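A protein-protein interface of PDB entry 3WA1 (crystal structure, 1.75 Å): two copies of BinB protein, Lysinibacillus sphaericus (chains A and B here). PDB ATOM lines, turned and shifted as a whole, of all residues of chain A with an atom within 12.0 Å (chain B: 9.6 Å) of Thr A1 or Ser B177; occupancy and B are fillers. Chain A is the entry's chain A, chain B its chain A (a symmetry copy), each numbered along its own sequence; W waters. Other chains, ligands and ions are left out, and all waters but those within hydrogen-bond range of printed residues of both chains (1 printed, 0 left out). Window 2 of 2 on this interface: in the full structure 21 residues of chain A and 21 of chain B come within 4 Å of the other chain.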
ATOM      1  N   THR A   1     -24.967   4.543 -12.462  1.00  0.00           N
ATOM      2  CA  THR A   1     -24.579   5.733 -11.618  1.00  0.00           C
ATOM      3  C   THR A   1     -23.080   6.043 -11.557  1.00  0.00           C
ATOM      4  O   THR A   1     -22.236   5.130 -11.573  1.00  0.00           O
ATOM      5  CB  THR A   1     -25.271   5.786 -10.224  1.00  0.00           C
ATOM      6  OG1 THR A   1     -25.537   4.466  -9.737  1.00  0.00           O
ATOM      7  CG2 THR A   1     -26.624   6.552 -10.305  1.00  0.00           C
ATOM      8  N   ASN A   2     -22.787   7.349 -11.499  1.00  0.00           N
ATOM      9  CA  ASN A   2     -21.406   7.911 -11.632  1.00  0.00           C
ATOM     10  C   ASN A   2     -20.589   7.955 -10.312  1.00  0.00           C
ATOM     11  O   ASN A   2     -19.365   8.083 -10.318  1.00  0.00           O
ATOM     12  CB  ASN A   2     -21.363   9.367 -12.263  1.00  0.00           C
ATOM     13  CG  ASN A   2     -22.641   9.776 -13.029  1.00  0.00           C
ATOM     14  OD1 ASN A   2     -23.427  10.613 -12.557  1.00  0.00           O
ATOM     15  ND2 ASN A   2     -22.822   9.236 -14.227  1.00  0.00           N
ATOM     16  N   TYR A   3     -21.293   7.901  -9.190  1.00  0.00           N
ATOM     17  CA  TYR A   3     -20.688   7.907  -7.897  1.00  0.00           C
ATOM     18  C   TYR A   3     -21.065   6.612  -7.163  1.00  0.00           C
ATOM     19  O   TYR A   3     -22.123   6.001  -7.478  1.00  0.00           O
ATOM     20  CB  TYR A   3     -21.253   9.115  -7.129  1.00  0.00           C
ATOM     21  CG  TYR A   3     -20.802  10.400  -7.727  1.00  0.00           C
ATOM     22  CD1 TYR A   3     -19.411  10.742  -7.710  1.00  0.00           C
ATOM     23  CD2 TYR A   3     -21.701  11.267  -8.350  1.00  0.00           C
ATOM     24  CE1 TYR A   3     -18.949  11.919  -8.260  1.00  0.00           C
ATOM     25  CE2 TYR A   3     -21.261  12.483  -8.906  1.00  0.00           C
ATOM     26  CZ  TYR A   3     -19.895  12.791  -8.884  1.00  0.00           C
ATOM     27  OH  TYR A   3     -19.435  13.967  -9.435  1.00  0.00           O
ATOM     28  N   PRO A   4     -20.249   6.225  -6.135  1.00  0.00           N
ATOM     29  CA  PRO A   4     -20.581   4.934  -5.428  1.00  0.00           C
ATOM     30  C   PRO A   4     -21.936   4.955  -4.786  1.00  0.00           C
ATOM     31  O   PRO A   4     -22.398   6.069  -4.438  1.00  0.00           O
ATOM     32  CB  PRO A   4     -19.561   4.869  -4.270  1.00  0.00           C
ATOM     33  CG  PRO A   4     -18.518   5.946  -4.567  1.00  0.00           C
ATOM     34  CD  PRO A   4     -19.037   6.888  -5.619  1.00  0.00           C
ATOM     35  N   LEU A   5     -22.527   3.770  -4.540  1.00  0.00           N
ATOM     36  CA  LEU A   5     -23.825   3.644  -3.842  1.00  0.00           C
ATOM     37  C   LEU A   5     -23.647   3.651  -2.353  1.00  0.00           C
ATOM     38  O   LEU A   5     -24.631   3.660  -1.592  1.00  0.00           O
ATOM     39  CB  LEU A   5     -24.600   2.348  -4.267  1.00  0.00           C
ATOM     40  CG  LEU A   5     -25.137   2.289  -5.757  1.00  0.00           C
ATOM     41  CD1 LEU A   5     -25.649   0.861  -6.101  1.00  0.00           C
ATOM     42  CD2 LEU A   5     -26.254   3.349  -5.946  1.00  0.00           C
ATOM     43  N   ASN A   6     -22.391   3.614  -1.918  1.00  0.00           N
ATOM     44  CA  ASN A   6     -22.053   3.651  -0.466  1.00  0.00           C
ATOM     45  C   ASN A   6     -21.261   4.919  -0.110  1.00  0.00           C
ATOM     46  O   ASN A   6     -20.670   5.560  -0.992  1.00  0.00           O
ATOM     47  CB  ASN A   6     -21.287   2.407   0.007  1.00  0.00           C
ATOM     48  CG  ASN A   6     -20.005   2.119  -0.776  1.00  0.00           C
ATOM     49  OD1 ASN A   6     -19.834   2.513  -1.954  1.00  0.00           O
ATOM     50  ND2 ASN A   6     -19.080   1.335  -0.121  1.00  0.00           N
ATOM     51  N   THR A   7     -21.244   5.275   1.162  1.00  0.00           N
ATOM     52  CA  THR A   7     -20.362   6.407   1.574  1.00  0.00           C
ATOM     53  C   THR A   7     -18.855   5.973   1.494  1.00  0.00           C
ATOM     54  O   THR A   7     -18.507   4.766   1.588  1.00  0.00           O
ATOM     55  CB  THR A   7     -20.698   6.885   2.989  1.00  0.00           C
ATOM     56  OG1 THR A   7     -20.771   5.757   3.857  1.00  0.00           O
ATOM     57  CG2 THR A   7     -22.025   7.620   3.014  1.00  0.00           C
ATOM     58  N   GLU B  18      -9.199   0.603 -11.313  1.00  0.00           N
ATOM     59  CA  GLU B  18     -10.485   0.996 -10.799  1.00  0.00           C
ATOM     60  C   GLU B  18     -11.483  -0.182 -10.539  1.00  0.00           C
ATOM     61  O   GLU B  18     -12.282  -0.176  -9.549  1.00  0.00           O
ATOM     62  CB  GLU B  18     -11.061   1.965 -11.856  1.00  0.00           C
ATOM     63  CG  GLU B  18     -12.413   2.479 -11.521  1.00  0.00           C
ATOM     64  CD  GLU B  18     -12.962   3.428 -12.606  1.00  0.00           C
ATOM     65  OE1 GLU B  18     -12.523   3.342 -13.786  1.00  0.00           O
ATOM     66  OE2 GLU B  18     -13.821   4.229 -12.278  1.00  0.00           O
ATOM     67  N   LYS B  22     -13.888  -1.358  -6.841  1.00  0.00           N
ATOM     68  CA  LYS B  22     -15.367  -1.080  -6.940  1.00  0.00           C
ATOM     69  C   LYS B  22     -16.079  -2.423  -7.131  1.00  0.00           C
ATOM     70  O   LYS B  22     -15.500  -3.322  -7.767  1.00  0.00           O
ATOM     71  CB  LYS B  22     -15.673  -0.202  -8.189  1.00  0.00           C
ATOM     72  CG  LYS B  22     -14.987   1.167  -7.999  1.00  0.00           C
ATOM     73  CD  LYS B  22     -15.327   2.097  -9.187  1.00  0.00           C
ATOM     74  CE  LYS B  22     -14.787   3.466  -8.820  1.00  0.00           C
ATOM     75  NZ  LYS B  22     -15.257   4.336  -9.961  1.00  0.00           N
ATOM     76  N   PHE B  23     -17.247  -2.590  -6.556  1.00  0.00           N
ATOM     77  CA  PHE B  23     -18.058  -3.818  -6.861  1.00  0.00           C
ATOM     78  C   PHE B  23     -19.104  -3.297  -7.873  1.00  0.00           C
ATOM     79  O   PHE B  23     -19.974  -2.500  -7.506  1.00  0.00           O
ATOM     80  CB  PHE B  23     -18.818  -4.209  -5.609  1.00  0.00           C
ATOM     81  CG  PHE B  23     -17.918  -4.716  -4.507  1.00  0.00           C
ATOM     82  CD1 PHE B  23     -17.642  -6.099  -4.389  1.00  0.00           C
ATOM     83  CD2 PHE B  23     -17.454  -3.801  -3.497  1.00  0.00           C
ATOM     84  CE1 PHE B  23     -16.812  -6.570  -3.374  1.00  0.00           C
ATOM     85  CE2 PHE B  23     -16.654  -4.290  -2.418  1.00  0.00           C
ATOM     86  CZ  PHE B  23     -16.335  -5.659  -2.372  1.00  0.00           C
ATOM     87  N   TYR B  24     -18.939  -3.671  -9.129  1.00  0.00           N
ATOM     88  CA  TYR B  24     -19.843  -3.252 -10.210  1.00  0.00           C
ATOM     89  C   TYR B  24     -20.942  -4.251 -10.509  1.00  0.00           C
ATOM     90  O   TYR B  24     -20.746  -5.470 -10.471  1.00  0.00           O
ATOM     91  CB  TYR B  24     -18.992  -3.185 -11.505  1.00  0.00           C
ATOM     92  CG  TYR B  24     -18.293  -1.824 -11.694  1.00  0.00           C
ATOM     93  CD1 TYR B  24     -19.061  -0.655 -12.040  1.00  0.00           C
ATOM     94  CD2 TYR B  24     -16.888  -1.717 -11.562  1.00  0.00           C
ATOM     95  CE1 TYR B  24     -18.437   0.561 -12.274  1.00  0.00           C
ATOM     96  CE2 TYR B  24     -16.272  -0.513 -11.791  1.00  0.00           C
ATOM     97  CZ  TYR B  24     -17.052   0.628 -12.112  1.00  0.00           C
ATOM     98  OH  TYR B  24     -16.417   1.855 -12.332  1.00  0.00           O
ATOM     99  N   ASN B  25     -22.115  -3.699 -10.867  1.00  0.00           N
ATOM    100  CA  ASN B  25     -23.261  -4.455 -11.439  1.00  0.00           C
ATOM    101  C   ASN B  25     -22.887  -4.649 -12.888  1.00  0.00           C
ATOM    102  O   ASN B  25     -22.647  -3.664 -13.566  1.00  0.00           O
ATOM    103  CB  ASN B  25     -24.447  -3.515 -11.338  1.00  0.00           C
ATOM    104  CG  ASN B  25     -25.766  -4.141 -11.719  1.00  0.00           C
ATOM    105  OD1 ASN B  25     -26.780  -3.438 -11.525  1.00  0.00           O
ATOM    106  ND2 ASN B  25     -25.805  -5.286 -12.231  1.00  0.00           N
ATOM    107  N   LEU B  26     -22.750  -5.885 -13.306  1.00  0.00           N
ATOM    108  CA  LEU B  26     -22.286  -6.226 -14.697  1.00  0.00           C
ATOM    109  C   LEU B  26     -23.538  -6.525 -15.540  1.00  0.00           C
ATOM    110  O   LEU B  26     -24.238  -7.550 -15.254  1.00  0.00           O
ATOM    111  CB  LEU B  26     -21.357  -7.425 -14.695  1.00  0.00           C
ATOM    112  CG  LEU B  26     -20.051  -7.215 -13.890  1.00  0.00           C
ATOM    113  CD1 LEU B  26     -19.181  -8.401 -14.244  1.00  0.00           C
ATOM    114  CD2 LEU B  26     -19.382  -5.943 -14.405  1.00  0.00           C
ATOM    115  N   LYS B  27     -23.837  -5.607 -16.478  1.00  0.00           N
ATOM    116  CA  LYS B  27     -25.035  -5.786 -17.389  1.00  0.00           C
ATOM    117  C   LYS B  27     -24.661  -6.273 -18.749  1.00  0.00           C
ATOM    118  O   LYS B  27     -23.576  -6.006 -19.206  1.00  0.00           O
ATOM    119  CB  LYS B  27     -25.722  -4.426 -17.544  1.00  0.00           C
ATOM    120  CG  LYS B  27     -26.328  -3.881 -16.244  1.00  0.00           C
ATOM    121  CD  LYS B  27     -27.658  -4.633 -15.938  1.00  0.00           C
ATOM    122  CE  LYS B  27     -28.443  -4.028 -14.793  1.00  0.00           C
ATOM    123  NZ  LYS B  27     -29.538  -4.977 -14.408  1.00  0.00           N
ATOM    124  N   LEU B  37     -25.743 -10.018 -14.589  1.00  0.00           N
ATOM    125  CA  LEU B  37     -25.536 -11.065 -13.592  1.00  0.00           C
ATOM    126  C   LEU B  37     -26.237 -10.805 -12.294  1.00  0.00           C
ATOM    127  O   LEU B  37     -26.281  -9.693 -11.770  1.00  0.00           O
ATOM    128  CB  LEU B  37     -24.000 -11.177 -13.409  1.00  0.00           C
ATOM    129  CG  LEU B  37     -23.228 -11.400 -14.722  1.00  0.00           C
ATOM    130  CD1 LEU B  37     -21.710 -11.651 -14.326  1.00  0.00           C
ATOM    131  CD2 LEU B  37     -23.741 -12.611 -15.548  1.00  0.00           C
ATOM    132  N   PRO B  63     -29.484  -7.803  -8.709  1.00  0.00           N
ATOM    133  CA  PRO B  63     -28.172  -7.845  -9.397  1.00  0.00           C
ATOM    134  C   PRO B  63     -27.035  -8.251  -8.367  1.00  0.00           C
ATOM    135  O   PRO B  63     -27.143  -7.947  -7.202  1.00  0.00           O
ATOM    136  CB  PRO B  63     -27.987  -6.410  -9.854  1.00  0.00           C
ATOM    137  CG  PRO B  63     -28.803  -5.588  -8.854  1.00  0.00           C
ATOM    138  CD  PRO B  63     -30.045  -6.432  -8.662  1.00  0.00           C
ATOM    139  N   ARG B  64     -25.966  -8.831  -8.868  1.00  0.00           N
ATOM    140  CA  ARG B  64     -24.715  -8.985  -8.106  1.00  0.00           C
ATOM    141  C   ARG B  64     -23.888  -7.748  -8.280  1.00  0.00           C
ATOM    142  O   ARG B  64     -23.955  -7.117  -9.340  1.00  0.00           O
ATOM    143  CB  ARG B  64     -23.945 -10.163  -8.679  1.00  0.00           C
ATOM    144  CG  ARG B  64     -24.552 -11.480  -8.187  1.00  0.00           C
ATOM    145  CD  ARG B  64     -23.906 -12.595  -9.020  1.00  0.00           C
ATOM    146  NE  ARG B  64     -24.322 -13.921  -8.544  1.00  0.00           N
ATOM    147  CZ  ARG B  64     -23.793 -14.562  -7.479  1.00  0.00           C
ATOM    148  NH1 ARG B  64     -22.748 -13.967  -6.809  1.00  0.00           N
ATOM    149  NH2 ARG B  64     -24.137 -15.839  -7.172  1.00  0.00           N
ATOM    150  N   PHE B  65     -23.020  -7.482  -7.283  1.00  0.00           N
ATOM    151  CA  PHE B  65     -22.031  -6.367  -7.311  1.00  0.00           C
ATOM    152  C   PHE B  65     -20.676  -7.008  -7.160  1.00  0.00           C
ATOM    153  O   PHE B  65     -20.468  -7.743  -6.191  1.00  0.00           O
ATOM    154  CB  PHE B  65     -22.398  -5.353  -6.210  1.00  0.00           C
ATOM    155  CG  PHE B  65     -23.580  -4.525  -6.594  1.00  0.00           C
ATOM    156  CD1 PHE B  65     -23.443  -3.349  -7.307  1.00  0.00           C
ATOM    157  CD2 PHE B  65     -24.876  -4.994  -6.246  1.00  0.00           C
ATOM    158  CE1 PHE B  65     -24.572  -2.576  -7.647  1.00  0.00           C
ATOM    159  CE2 PHE B  65     -26.023  -4.239  -6.636  1.00  0.00           C
ATOM    160  CZ  PHE B  65     -25.830  -3.065  -7.271  1.00  0.00           C
ATOM    161  N   LEU B  66     -19.839  -6.888  -8.174  1.00  0.00           N
ATOM    162  CA  LEU B  66     -18.727  -7.832  -8.307  1.00  0.00           C
ATOM    163  C   LEU B  66     -17.449  -7.057  -8.371  1.00  0.00           C
ATOM    164  O   LEU B  66     -17.337  -6.137  -9.192  1.00  0.00           O
ATOM    165  CB  LEU B  66     -18.852  -8.640  -9.584  1.00  0.00           C
ATOM    166  CG  LEU B  66     -20.126  -9.520  -9.569  1.00  0.00           C
ATOM    167  CD1 LEU B  66     -20.366  -9.957 -11.031  1.00  0.00           C
ATOM    168  CD2 LEU B  66     -19.971 -10.792  -8.740  1.00  0.00           C
ATOM    169  N   ILE B  67     -16.453  -7.452  -7.557  1.00  0.00           N
ATOM    170  CA  ILE B  67     -15.153  -6.779  -7.677  1.00  0.00           C
ATOM    171  C   ILE B  67     -14.247  -7.711  -8.441  1.00  0.00           C
ATOM    172  O   ILE B  67     -14.438  -8.904  -8.421  1.00  0.00           O
ATOM    173  CB  ILE B  67     -14.529  -6.477  -6.251  1.00  0.00           C
ATOM    174  CG1 ILE B  67     -13.245  -5.675  -6.343  1.00  0.00           C
ATOM    175  CG2 ILE B  67     -14.394  -7.747  -5.430  1.00  0.00           C
ATOM    176  CD1 ILE B  67     -13.061  -4.951  -5.012  1.00  0.00           C
ATOM    177  N   ARG B  68     -13.295  -7.138  -9.179  1.00  0.00           N
ATOM    178  CA  ARG B  68     -12.302  -7.893  -9.928  1.00  0.00           C
ATOM    179  C   ARG B  68     -10.910  -7.729  -9.265  1.00  0.00           C
ATOM    180  O   ARG B  68     -10.263  -6.689  -9.417  1.00  0.00           O
ATOM    181  CB  ARG B  68     -12.324  -7.418 -11.405  1.00  0.00           C
ATOM    182  CG  ARG B  68     -13.480  -8.136 -12.118  1.00  0.00           C
ATOM    183  CD  ARG B  68     -13.939  -7.401 -13.438  1.00  0.00           C
ATOM    184  NE  ARG B  68     -14.690  -6.211 -13.051  1.00  0.00           N
ATOM    185  CZ  ARG B  68     -15.335  -5.422 -13.909  1.00  0.00           C
ATOM    186  NH1 ARG B  68     -15.192  -5.670 -15.230  1.00  0.00           N
ATOM    187  NH2 ARG B  68     -16.026  -4.396 -13.444  1.00  0.00           N
ATOM    188  N   ARG B  81     -19.946  -9.119  -3.630  1.00  0.00           N
ATOM    189  CA  ARG B  81     -19.993  -8.248  -2.441  1.00  0.00           C
ATOM    190  C   ARG B  81     -20.671  -8.854  -1.252  1.00  0.00           C
ATOM    191  O   ARG B  81     -20.360  -8.503  -0.084  1.00  0.00           O
ATOM    192  CB  ARG B  81     -20.612  -6.874  -2.804  1.00  0.00           C
ATOM    193  CG  ARG B  81     -20.488  -5.781  -1.693  1.00  0.00           C
ATOM    194  CD  ARG B  81     -20.866  -4.376  -2.241  1.00  0.00           C
ATOM    195  NE  ARG B  81     -20.445  -3.347  -1.257  1.00  0.00           N
ATOM    196  CZ  ARG B  81     -21.266  -2.794  -0.381  1.00  0.00           C
ATOM    197  NH1 ARG B  81     -22.562  -3.094  -0.341  1.00  0.00           N
ATOM    198  NH2 ARG B  81     -20.771  -1.860   0.415  1.00  0.00           N
ATOM    199  N   VAL B 174     -21.058  -4.687 -19.764  1.00  0.00           N
ATOM    200  CA  VAL B 174     -20.690  -3.327 -19.467  1.00  0.00           C
ATOM    201  C   VAL B 174     -20.839  -3.125 -17.957  1.00  0.00           C
ATOM    202  O   VAL B 174     -21.620  -3.821 -17.301  1.00  0.00           O
ATOM    203  CB  VAL B 174     -21.611  -2.315 -20.198  1.00  0.00           C
ATOM    204  CG1 VAL B 174     -21.320  -2.374 -21.721  1.00  0.00           C
ATOM    205  CG2 VAL B 174     -23.086  -2.562 -19.888  1.00  0.00           C
ATOM    206  N   ASN B 175     -20.096  -2.171 -17.424  1.00  0.00           N
ATOM    207  CA  ASN B 175     -20.273  -1.810 -16.039  1.00  0.00           C
ATOM    208  C   ASN B 175     -21.472  -0.882 -15.857  1.00  0.00           C
ATOM    209  O   ASN B 175     -21.692   0.007 -16.690  1.00  0.00           O
ATOM    210  CB  ASN B 175     -19.062  -1.018 -15.619  1.00  0.00           C
ATOM    211  CG  ASN B 175     -17.812  -1.874 -15.451  1.00  0.00           C
ATOM    212  OD1 ASN B 175     -17.883  -3.100 -15.093  1.00  0.00           O
ATOM    213  ND2 ASN B 175     -16.649  -1.265 -15.806  1.00  0.00           N
ATOM    214  N   SER B 176     -22.194  -1.047 -14.745  1.00  0.00           N
ATOM    215  CA  SER B 176     -23.337  -0.216 -14.376  1.00  0.00           C
ATOM    216  C   SER B 176     -23.072   0.463 -13.021  1.00  0.00           C
ATOM    217  O   SER B 176     -21.958   1.011 -12.864  1.00  0.00           O
ATOM    218  CB  SER B 176     -24.635  -1.061 -14.376  1.00  0.00           C
ATOM    219  OG  SER B 176     -25.739  -0.164 -14.407  1.00  0.00           O
ATOM    220  N   SER B 177     -24.028   0.352 -12.098  1.00  0.00           N
ATOM    221  CA  SER B 177     -23.941   0.989 -10.779  1.00  0.00           C
ATOM    222  C   SER B 177     -22.795   0.255  -9.972  1.00  0.00           C
ATOM    223  O   SER B 177     -22.336  -0.856 -10.376  1.00  0.00           O
ATOM    224  CB  SER B 177     -25.271   0.988 -10.052  1.00  0.00           C
ATOM    225  OG  SER B 177     -25.761  -0.342  -9.839  1.00  0.00           O
ATOM    226  N   PHE B 178     -22.364   0.878  -8.871  1.00  0.00           N
ATOM    227  CA  PHE B 178     -21.256   0.253  -8.082  1.00  0.00           C
ATOM    228  C   PHE B 178     -21.202   0.714  -6.672  1.00  0.00           C
ATOM    229  O   PHE B 178     -21.819   1.750  -6.336  1.00  0.00           O
ATOM    230  CB  PHE B 178     -19.879   0.521  -8.735  1.00  0.00           C
ATOM    231  CG  PHE B 178     -19.410   1.941  -8.663  1.00  0.00           C
ATOM    232  CD1 PHE B 178     -19.773   2.885  -9.668  1.00  0.00           C
ATOM    233  CD2 PHE B 178     -18.515   2.327  -7.656  1.00  0.00           C
ATOM    234  CE1 PHE B 178     -19.339   4.215  -9.578  1.00  0.00           C
ATOM    235  CE2 PHE B 178     -18.111   3.652  -7.556  1.00  0.00           C
ATOM    236  CZ  PHE B 178     -18.452   4.564  -8.536  1.00  0.00           C
ATOM    237  N   TYR B 179     -20.518  -0.099  -5.835  1.00  0.00           N
ATOM    238  CA  TYR B 179     -20.207   0.315  -4.454  1.00  0.00           C
ATOM    239  C   TYR B 179     -18.713   0.410  -4.405  1.00  0.00           C
ATOM    240  O   TYR B 179     -18.042  -0.412  -5.017  1.00  0.00           O
ATOM    241  CB  TYR B 179     -20.634  -0.802  -3.481  1.00  0.00           C
ATOM    242  CG  TYR B 179     -22.112  -0.991  -3.351  1.00  0.00           C
ATOM    243  CD1 TYR B 179     -22.826  -1.813  -4.253  1.00  0.00           C
ATOM    244  CD2 TYR B 179     -22.846  -0.310  -2.345  1.00  0.00           C
ATOM    245  CE1 TYR B 179     -24.184  -1.936  -4.115  1.00  0.00           C
ATOM    246  CE2 TYR B 179     -24.198  -0.520  -2.173  1.00  0.00           C
ATOM    247  CZ  TYR B 179     -24.855  -1.257  -3.090  1.00  0.00           C
ATOM    248  OH  TYR B 179     -26.192  -1.470  -2.988  1.00  0.00           O
ATOM    249  N   ALA B 180     -18.173   1.396  -3.661  1.00  0.00           N
ATOM    250  CA  ALA B 180     -16.742   1.474  -3.503  1.00  0.00           C
ATOM    251  C   ALA B 180     -16.232   0.366  -2.548  1.00  0.00           C
ATOM    252  O   ALA B 180     -16.871   0.088  -1.507  1.00  0.00           O
ATOM    253  CB  ALA B 180     -16.377   2.848  -2.865  1.00  0.00           C
HETATM  254  O   HOH W   1     -23.242   3.709  -8.790  1.00  0.00           O
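N of Leu A5 is in hydrogen-bond range of O of Phe B178.
OD1 of Asn A6 is in hydrogen-bond range of N of Ala B180.
N of Phe B23 lies within hydrogen-bond range of O of Tyr B179 (2.8 Å).
N of Asn B25 is in hydrogen-bond range of O of Ser B177 (2.9 Å).
O of Phe B65 lies within hydrogen-bond range of N of Arg B81, 3.0 Å away.
Among the printed residues, pairs that only touch across the chains: Thr A1 with Ser B177 (3.5 Å), Thr A1 with Phe B178 (3.6 Å), Asn A2 with Phe B178 (3.9 Å), Tyr A3 with Phe B178 (3.6 Å), Pro A4 with Phe B178 (3.4 Å), Pro A4 with Ala B180 (3.8 Å), Leu A5 with Phe B65 (3.9 Å), Leu A5 with Ser B177 (3.9 Å), Leu A5 with Tyr B179 (3.6 Å), Asn A6 with Arg B81 (3.7 Å) and Asn A6 with Tyr B179 (3.3 Å).
Thr A1 touches two residues of chain B.
Of chain B, only Phe B178 comes within 4 Å of Asn A2.
Printed residues of chain B within 4 Å of Tyr A3: Phe B178 (3.6 Å).
Of the printed residues of chain B, Pro A4 touches Phe B178 (3.4 Å) and Ala B180 (3.8 Å).
Tyr B24 touches none of the printed residues of chain A.
Pro B63 touches none of the printed residues of chain A.
Arg B68 touches none of the printed residues of chain A.
Of the printed residues of chain A, Arg B81 touches Asn A6.
Asn B175 touches none of the printed residues of chain A.
No residue of chain A comes within 4 Å of Ser B176.
Of the printed residues of chain A, Ser B177 touches Thr A1 and Leu A5.
The nearest residue of chain B that does not touch Thr A1 is Ser B176 (4.3 Å).
The nearest residue of chain A that does not touch Ser B177 is Tyr A3 (6.3 Å).
Of the 22 printed residues of chain B, 6 touch a printed residue of chain A.
Hydrophobic or aromatic side chains of chain B within 4 Å of the printed part of chain A: Phe B65, Phe B178, Tyr B179 and Ala B180.
Hydrophobic or aromatic side chains of chain A that line the printed part of chain B: Pro A4 and Leu A5.
Among the printed residues, 13 pairs touch across the chains.
Among the printed residues, no Asp or Glu carboxylate lies within 4 Å of a Lys or Arg side-chain nitrogen of the other chain.
No position is printed for both chains.
Of the 13 pairs that touch across the chains among the printed residues, none has its exchanged pair printed and touching as well.
Water W1 lies within hydrogen-bond range of OG1 of Thr A1 (2.6 Å), O of Tyr A3 (2.9 Å) and N of Phe B178 (3.0 Å).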
